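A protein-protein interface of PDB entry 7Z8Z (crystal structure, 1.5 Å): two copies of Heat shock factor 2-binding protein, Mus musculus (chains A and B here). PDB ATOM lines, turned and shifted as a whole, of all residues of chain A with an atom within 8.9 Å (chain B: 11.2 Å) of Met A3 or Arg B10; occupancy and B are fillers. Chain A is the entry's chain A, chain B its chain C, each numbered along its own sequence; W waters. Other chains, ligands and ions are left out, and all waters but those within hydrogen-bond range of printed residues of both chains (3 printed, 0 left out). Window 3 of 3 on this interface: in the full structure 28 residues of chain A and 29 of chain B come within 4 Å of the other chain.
OG1 of Thr B18 sits at hydrogen-bond distance from O of Leu B14 (3.2 Å).
Hydrophobic or aromatic side chains of chain B that line the printed part of chain A: Val B7 and Leu B14. Of the 7 printed residues of chain A, 7 touch a printed residue of chain B. Printed residues of chain A that touch a printed residue of chain B: Met A3, Glu A4, Glu A5, Phe A6, Val A7, Lys A8 and Val A9. Along chain A the printed residues that touch a printed residue of chain B span positions 3 to 9. Among the printed residues, no Asp or Glu carboxylate lies within 4 Å of a Lys or Arg side-chain nitrogen of the other chain.
The backbone carbonyl oxygen (O) of Val A9 is in hydrogen-bond range of the backbone NH (N) of Val B7, 2.8 Å away. The backbone NH (N) of Val A7 lies within hydrogen-bond range of the backbone carbonyl oxygen (O) of Val B9 (2.8 Å). O of Glu A4 is in hydrogen-bond range of NH1 of Arg B10, 2.7 Å away. N of Lys B11 lies within hydrogen-bond range of O of Glu A5 (2.8 Å). The guanidinium group (NH1) of Arg B10 sits at hydrogen-bond distance from the side-chain sulfur (SD) of Met A3.
Val A7 touches Lys B8, and with the chains exchanged Lys A8 touches Val B7. Val A7 touches Val B9, and with the chains exchanged Val A9 touches Val B7. Positions printed for both chains: 7, 8 and 9.
Water W1 bridges the side-chain amino group (NZ) of Lys B12 (2.5 Å) and the side-chain carboxylate (OE2) of Glu A4 (2.7 Å). Water W2 lies within hydrogen-bond range of the backbone carbonyl oxygen of Glu A5, the backbone NH of Lys B12 and the backbone NH of Lys B11. Water W3 lies within hydrogen-bond range of N of Glu A4 and NH1 of Arg B10.
Met A3 touches just one residue of chain B: Arg B10. Of chain B, only Arg B10 (2.7 Å) and Lys B12 (3.5 Å) come within 4 Å of Glu A4. Phe A6 touches three residues of chain B. Val A7 touches just these residues of chain B: Lys B8 (3.3 Å), Val B9 (2.8 Å), Lys B11 (3.8 Å) and Leu B14 (3.97 Å). Of the printed residues of chain A, Leu B14 touches Val A7. Of the printed residues of chain A, Lys B8 touches Phe A6 and Val A7. Of the printed residues of chain B, Lys A8 touches Val B7. Arg B16 touches none of the printed residues of chain A. The nearest residue of chain B that does not touch Met A3 is Lys B8 (6.3 Å). The nearest residue of chain A that does not touch Arg B10 is Val A7 (4.8 Å). The nearest printed residue of chain A that does not touch Lys B8 is Lys A8 (4.4 Å).
CD of Lys B12 touches OE2 of Glu A4 (3.5 Å). Arg B10 touches Glu A5 (CA to O, 3.5 Å). Lys B8 touches Phe A6. CA of Phe A6 touches O of Val B9 (3.4 Å). Phe A6 touches Arg B10 (CZ to CZ, 3.2 Å). O of Val A7 touches CA of Lys B8, at 3.3 Å. CG1 of Val A7 touches CG of Lys B11, 3.8 Å away. Val A7 touches Leu B14 (CG2 to CD2, 3.97 Å). O of Val B7 touches CA of Lys A8 (3.2 Å).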
ATOM      1  N   MET A   3     -20.832 -35.701  17.104  1.00  0.00           N
ATOM      2  CA  MET A   3     -19.634 -35.562  17.925  1.00  0.00           C
ATOM      3  C   MET A   3     -19.809 -34.443  18.952  1.00  0.00           C
ATOM      4  O   MET A   3     -20.787 -33.696  18.906  1.00  0.00           O
ATOM      5  CB  MET A   3     -18.410 -35.286  17.046  1.00  0.00           C
ATOM      6  CG  MET A   3     -18.400 -33.918  16.384  1.00  0.00           C
ATOM      7  SD  MET A   3     -16.841 -33.562  15.532  1.00  0.00           S
ATOM      8  CE  MET A   3     -17.073 -31.838  15.090  1.00  0.00           C
ATOM      9  N   GLU A   4     -18.852 -34.330  19.872  1.00  0.00           N
ATOM     10  CA  GLU A   4     -18.865 -33.253  20.852  1.00  0.00           C
ATOM     11  C   GLU A   4     -18.399 -31.953  20.211  1.00  0.00           C
ATOM     12  O   GLU A   4     -17.426 -31.926  19.451  1.00  0.00           O
ATOM     13  CB  GLU A   4     -17.979 -33.608  22.043  1.00  0.00           C
ATOM     14  CG  GLU A   4     -18.604 -34.630  22.988  1.00  0.00           C
ATOM     15  CD  GLU A   4     -17.782 -34.824  24.248  1.00  0.00           C
ATOM     16  OE1 GLU A   4     -16.544 -35.000  24.138  1.00  0.00           O
ATOM     17  OE2 GLU A   4     -18.371 -34.786  25.350  1.00  0.00           O
ATOM     18  N   GLU A   5     -19.097 -30.866  20.534  1.00  0.00           N
ATOM     19  CA  GLU A   5     -18.931 -29.614  19.805  1.00  0.00           C
ATOM     20  C   GLU A   5     -17.590 -28.973  20.115  1.00  0.00           C
ATOM     21  O   GLU A   5     -17.087 -29.065  21.236  1.00  0.00           O
ATOM     22  CB  GLU A   5     -20.076 -28.665  20.171  1.00  0.00           C
ATOM     23  CG  GLU A   5     -20.076 -27.308  19.488  1.00  0.00           C
ATOM     24  CD  GLU A   5     -21.283 -26.467  19.891  1.00  0.00           C
ATOM     25  OE1 GLU A   5     -22.169 -27.001  20.596  1.00  0.00           O
ATOM     26  OE2 GLU A   5     -21.350 -25.278  19.506  1.00  0.00           O
ATOM     27  N   PHE A   6     -17.014 -28.317  19.109  1.00  0.00           N
ATOM     28  CA  PHE A   6     -15.822 -27.506  19.268  1.00  0.00           C
ATOM     29  C   PHE A   6     -16.195 -26.037  19.441  1.00  0.00           C
ATOM     30  O   PHE A   6     -17.223 -25.574  18.938  1.00  0.00           O
ATOM     31  CB  PHE A   6     -14.900 -27.610  18.049  1.00  0.00           C
ATOM     32  CG  PHE A   6     -14.106 -28.874  17.975  1.00  0.00           C
ATOM     33  CD1 PHE A   6     -12.966 -29.020  18.737  1.00  0.00           C
ATOM     34  CD2 PHE A   6     -14.486 -29.906  17.137  1.00  0.00           C
ATOM     35  CE1 PHE A   6     -12.216 -30.173  18.669  1.00  0.00           C
ATOM     36  CE2 PHE A   6     -13.739 -31.062  17.061  1.00  0.00           C
ATOM     37  CZ  PHE A   6     -12.601 -31.194  17.833  1.00  0.00           C
ATOM     38  N   VAL A   7     -15.334 -25.306  20.145  1.00  0.00           N
ATOM     39  CA  VAL A   7     -15.289 -23.850  20.098  1.00  0.00           C
ATOM     40  C   VAL A   7     -13.896 -23.470  19.610  1.00  0.00           C
ATOM     41  O   VAL A   7     -12.964 -24.274  19.655  1.00  0.00           O
ATOM     42  CB  VAL A   7     -15.606 -23.190  21.452  1.00  0.00           C
ATOM     43  CG1 VAL A   7     -17.057 -23.515  21.849  1.00  0.00           C
ATOM     44  CG2 VAL A   7     -14.637 -23.641  22.522  1.00  0.00           C
ATOM     45  N   LYS A   8     -13.755 -22.243  19.124  1.00  0.00           N
ATOM     46  CA  LYS A   8     -12.460 -21.755  18.672  1.00  0.00           C
ATOM     47  C   LYS A   8     -11.948 -20.673  19.617  1.00  0.00           C
ATOM     48  O   LYS A   8     -12.719 -19.941  20.249  1.00  0.00           O
ATOM     49  CB  LYS A   8     -12.519 -21.245  17.218  1.00  0.00           C
ATOM     50  CG  LYS A   8     -13.361 -20.021  16.971  1.00  0.00           C
ATOM     51  CD  LYS A   8     -13.386 -19.680  15.463  1.00  0.00           C
ATOM     52  CE  LYS A   8     -14.136 -18.384  15.208  1.00  0.00           C
ATOM     53  NZ  LYS A   8     -14.295 -18.129  13.741  1.00  0.00           N
ATOM     54  N   VAL A   9     -10.617 -20.601  19.715  1.00  0.00           N
ATOM     55  CA  VAL A   9      -9.905 -19.686  20.600  1.00  0.00           C
ATOM     56  C   VAL A   9      -8.653 -19.205  19.872  1.00  0.00           C
ATOM     57  O   VAL A   9      -7.931 -20.009  19.277  1.00  0.00           O
ATOM     58  CB  VAL A   9      -9.512 -20.374  21.924  1.00  0.00           C
ATOM     59  CG1 VAL A   9      -8.684 -19.470  22.803  1.00  0.00           C
ATOM     60  CG2 VAL A   9     -10.762 -20.860  22.676  1.00  0.00           C
ATOM     61  N   VAL B   7      -7.179 -21.876  17.306  1.00  0.00           N
ATOM     62  CA  VAL B   7      -7.193 -23.305  17.581  1.00  0.00           C
ATOM     63  C   VAL B   7      -8.611 -23.678  18.007  1.00  0.00           C
ATOM     64  O   VAL B   7      -9.413 -22.827  18.411  1.00  0.00           O
ATOM     65  CB  VAL B   7      -6.172 -23.705  18.659  1.00  0.00           C
ATOM     66  CG1 VAL B   7      -4.771 -23.449  18.150  1.00  0.00           C
ATOM     67  CG2 VAL B   7      -6.427 -22.937  19.942  1.00  0.00           C
ATOM     68  N   LYS B   8      -8.935 -24.959  17.885  1.00  0.00           N
ATOM     69  CA  LYS B   8     -10.219 -25.471  18.342  1.00  0.00           C
ATOM     70  C   LYS B   8     -10.030 -26.304  19.605  1.00  0.00           C
ATOM     71  O   LYS B   8      -8.980 -26.925  19.820  1.00  0.00           O
ATOM     72  CB  LYS B   8     -10.922 -26.293  17.252  1.00  0.00           C
ATOM     73  CG  LYS B   8     -10.219 -27.570  16.821  1.00  0.00           C
ATOM     74  CD  LYS B   8     -11.006 -28.268  15.700  1.00  0.00           C
ATOM     75  CE  LYS B   8     -10.339 -29.567  15.298  1.00  0.00           C
ATOM     76  NZ  LYS B   8     -11.023 -30.180  14.127  1.00  0.00           N
ATOM     77  N   VAL B   9     -11.052 -26.264  20.452  1.00  0.00           N
ATOM     78  CA  VAL B   9     -11.091 -26.986  21.718  1.00  0.00           C
ATOM     79  C   VAL B   9     -12.508 -27.516  21.923  1.00  0.00           C
ATOM     80  O   VAL B   9     -13.490 -26.799  21.694  1.00  0.00           O
ATOM     81  CB  VAL B   9     -10.702 -26.081  22.904  1.00  0.00           C
ATOM     82  CG1 VAL B   9     -10.859 -26.823  24.236  1.00  0.00           C
ATOM     83  CG2 VAL B   9      -9.275 -25.546  22.744  1.00  0.00           C
ATOM     84  N   ARG B  10     -12.625 -28.756  22.399  1.00  0.00           N
ATOM     85  CA  ARG B  10     -13.947 -29.266  22.729  1.00  0.00           C
ATOM     86  C   ARG B  10     -14.584 -28.344  23.765  1.00  0.00           C
ATOM     87  O   ARG B  10     -13.962 -28.009  24.785  1.00  0.00           O
ATOM     88  CB  ARG B  10     -13.877 -30.698  23.258  1.00  0.00           C
ATOM     89  CG  ARG B  10     -13.281 -31.686  22.302  1.00  0.00           C
ATOM     90  CD  ARG B  10     -14.196 -32.109  21.175  1.00  0.00           C
ATOM     91  NE  ARG B  10     -13.524 -33.099  20.333  1.00  0.00           N
ATOM     92  CZ  ARG B  10     -14.066 -33.688  19.278  1.00  0.00           C
ATOM     93  NH1 ARG B  10     -15.298 -33.410  18.890  1.00  0.00           N
ATOM     94  NH2 ARG B  10     -13.346 -34.568  18.586  1.00  0.00           N
ATOM     95  N   LYS B  11     -15.837 -27.955  23.494  1.00  0.00           N
ATOM     96  CA  LYS B  11     -16.551 -26.999  24.333  1.00  0.00           C
ATOM     97  C   LYS B  11     -16.636 -27.470  25.776  1.00  0.00           C
ATOM     98  O   LYS B  11     -16.454 -26.673  26.704  1.00  0.00           O
ATOM     99  CB  LYS B  11     -17.948 -26.768  23.740  1.00  0.00           C
ATOM    100  CG  LYS B  11     -18.799 -25.733  24.427  1.00  0.00           C
ATOM    101  CD  LYS B  11     -20.089 -25.509  23.655  1.00  0.00           C
ATOM    102  CE  LYS B  11     -20.805 -24.256  24.130  1.00  0.00           C
ATOM    103  NZ  LYS B  11     -22.000 -23.943  23.286  1.00  0.00           N
ATOM    104  N   LYS B  12     -16.923 -28.758  25.988  1.00  0.00           N
ATOM    105  CA  LYS B  12     -17.082 -29.240  27.349  1.00  0.00           C
ATOM    106  C   LYS B  12     -15.774 -29.177  28.122  1.00  0.00           C
ATOM    107  O   LYS B  12     -15.788 -28.954  29.333  1.00  0.00           O
ATOM    108  CB  LYS B  12     -17.640 -30.664  27.336  1.00  0.00           C
ATOM    109  CG  LYS B  12     -19.103 -30.758  26.944  1.00  0.00           C
ATOM    110  CD  LYS B  12     -19.658 -32.155  27.198  1.00  0.00           C
ATOM    111  CE  LYS B  12     -21.156 -32.215  26.914  1.00  0.00           C
ATOM    112  NZ  LYS B  12     -21.730 -33.556  27.231  1.00  0.00           N
ATOM    113  N   ASP B  13     -14.635 -29.363  27.450  1.00  0.00           N
ATOM    114  CA  ASP B  13     -13.360 -29.303  28.150  1.00  0.00           C
ATOM    115  C   ASP B  13     -13.037 -27.875  28.556  1.00  0.00           C
ATOM    116  O   ASP B  13     -12.504 -27.637  29.644  1.00  0.00           O
ATOM    117  CB  ASP B  13     -12.266 -29.912  27.277  1.00  0.00           C
ATOM    118  CG  ASP B  13     -12.444 -31.416  27.118  1.00  0.00           C
ATOM    119  OD1 ASP B  13     -12.260 -32.130  28.121  1.00  0.00           O
ATOM    120  OD2 ASP B  13     -12.797 -31.865  26.019  1.00  0.00           O
ATOM    121  N   LEU B  14     -13.355 -26.901  27.703  1.00  0.00           N
ATOM    122  CA  LEU B  14     -13.149 -25.508  28.096  1.00  0.00           C
ATOM    123  C   LEU B  14     -14.066 -25.126  29.257  1.00  0.00           C
ATOM    124  O   LEU B  14     -13.677 -24.352  30.144  1.00  0.00           O
ATOM    125  CB  LEU B  14     -13.364 -24.587  26.902  1.00  0.00           C
ATOM    126  CG  LEU B  14     -13.020 -23.125  27.219  1.00  0.00           C
ATOM    127  CD1 LEU B  14     -11.588 -22.938  27.655  1.00  0.00           C
ATOM    128  CD2 LEU B  14     -13.322 -22.237  26.000  1.00  0.00           C
ATOM    129  N   GLU B  15     -15.289 -25.673  29.282  1.00  0.00           N
ATOM    130  CA  GLU B  15     -16.189 -25.440  30.406  1.00  0.00           C
ATOM    131  C   GLU B  15     -15.587 -25.982  31.698  1.00  0.00           C
ATOM    132  O   GLU B  15     -15.662 -25.337  32.751  1.00  0.00           O
ATOM    133  CB  GLU B  15     -17.559 -26.077  30.125  1.00  0.00           C
ATOM    134  CG  GLU B  15     -18.547 -25.991  31.275  1.00  0.00           C
ATOM    135  CD  GLU B  15     -19.934 -26.496  30.899  1.00  0.00           C
ATOM    136  OE1 GLU B  15     -20.033 -27.591  30.309  1.00  0.00           O
ATOM    137  OE2 GLU B  15     -20.923 -25.786  31.178  1.00  0.00           O
ATOM    138  N   ARG B  16     -14.987 -27.174  31.638  1.00  0.00           N
ATOM    139  CA  ARG B  16     -14.323 -27.723  32.816  1.00  0.00           C
ATOM    140  C   ARG B  16     -13.206 -26.806  33.291  1.00  0.00           C
ATOM    141  O   ARG B  16     -13.033 -26.593  34.499  1.00  0.00           O
ATOM    142  CB  ARG B  16     -13.767 -29.112  32.497  1.00  0.00           C
ATOM    143  CG  ARG B  16     -14.793 -30.206  32.356  1.00  0.00           C
ATOM    144  CD  ARG B  16     -15.325 -30.656  33.723  1.00  0.00           C
ATOM    145  NE  ARG B  16     -14.250 -31.175  34.559  1.00  0.00           N
ATOM    146  CZ  ARG B  16     -13.777 -30.559  35.632  1.00  0.00           C
ATOM    147  NH1 ARG B  16     -14.267 -29.400  36.041  1.00  0.00           N
ATOM    148  NH2 ARG B  16     -12.770 -31.109  36.303  1.00  0.00           N
ATOM    149  N   LEU B  17     -12.416 -26.274  32.354  1.00  0.00           N
ATOM    150  CA  LEU B  17     -11.317 -25.394  32.737  1.00  0.00           C
ATOM    151  C   LEU B  17     -11.853 -24.150  33.430  1.00  0.00           C
ATOM    152  O   LEU B  17     -11.332 -23.740  34.479  1.00  0.00           O
ATOM    153  CB  LEU B  17     -10.478 -25.023  31.515  1.00  0.00           C
ATOM    154  CG  LEU B  17      -9.210 -24.216  31.800  1.00  0.00           C
ATOM    155  CD1 LEU B  17      -8.277 -24.957  32.725  1.00  0.00           C
ATOM    156  CD2 LEU B  17      -8.539 -23.906  30.480  1.00  0.00           C
ATOM    157  N   THR B  18     -12.916 -23.552  32.876  1.00  0.00           N
ATOM    158  CA  THR B  18     -13.509 -22.380  33.503  1.00  0.00           C
ATOM    159  C   THR B  18     -13.951 -22.697  34.923  1.00  0.00           C
ATOM    160  O   THR B  18     -13.712 -21.908  35.843  1.00  0.00           O
ATOM    161  CB  THR B  18     -14.690 -21.870  32.679  1.00  0.00           C
ATOM    162  OG1 THR B  18     -14.235 -21.494  31.377  1.00  0.00           O
ATOM    163  CG2 THR B  18     -15.331 -20.668  33.351  1.00  0.00           C
ATOM    164  N   THR B  19     -14.581 -23.857  35.126  1.00  0.00           N
ATOM    165  CA  THR B  19     -15.038 -24.218  36.465  1.00  0.00           C
ATOM    166  C   THR B  19     -13.873 -24.260  37.443  1.00  0.00           C
ATOM    167  O   THR B  19     -13.967 -23.749  38.568  1.00  0.00           O
ATOM    168  CB  THR B  19     -15.750 -25.573  36.434  1.00  0.00           C
ATOM    169  OG1 THR B  19     -16.876 -25.497  35.562  1.00  0.00           O
ATOM    170  CG2 THR B  19     -16.205 -25.990  37.826  1.00  0.00           C
HETATM  171  O   HOH W   1     -21.058 -35.220  25.511  1.00  0.00           O
HETATM  172  O   HOH W   2     -17.714 -30.503  23.724  1.00  0.00           O
HETATM  173  O   HOH W   3     -16.703 -36.398  19.819  1.00  0.00           O
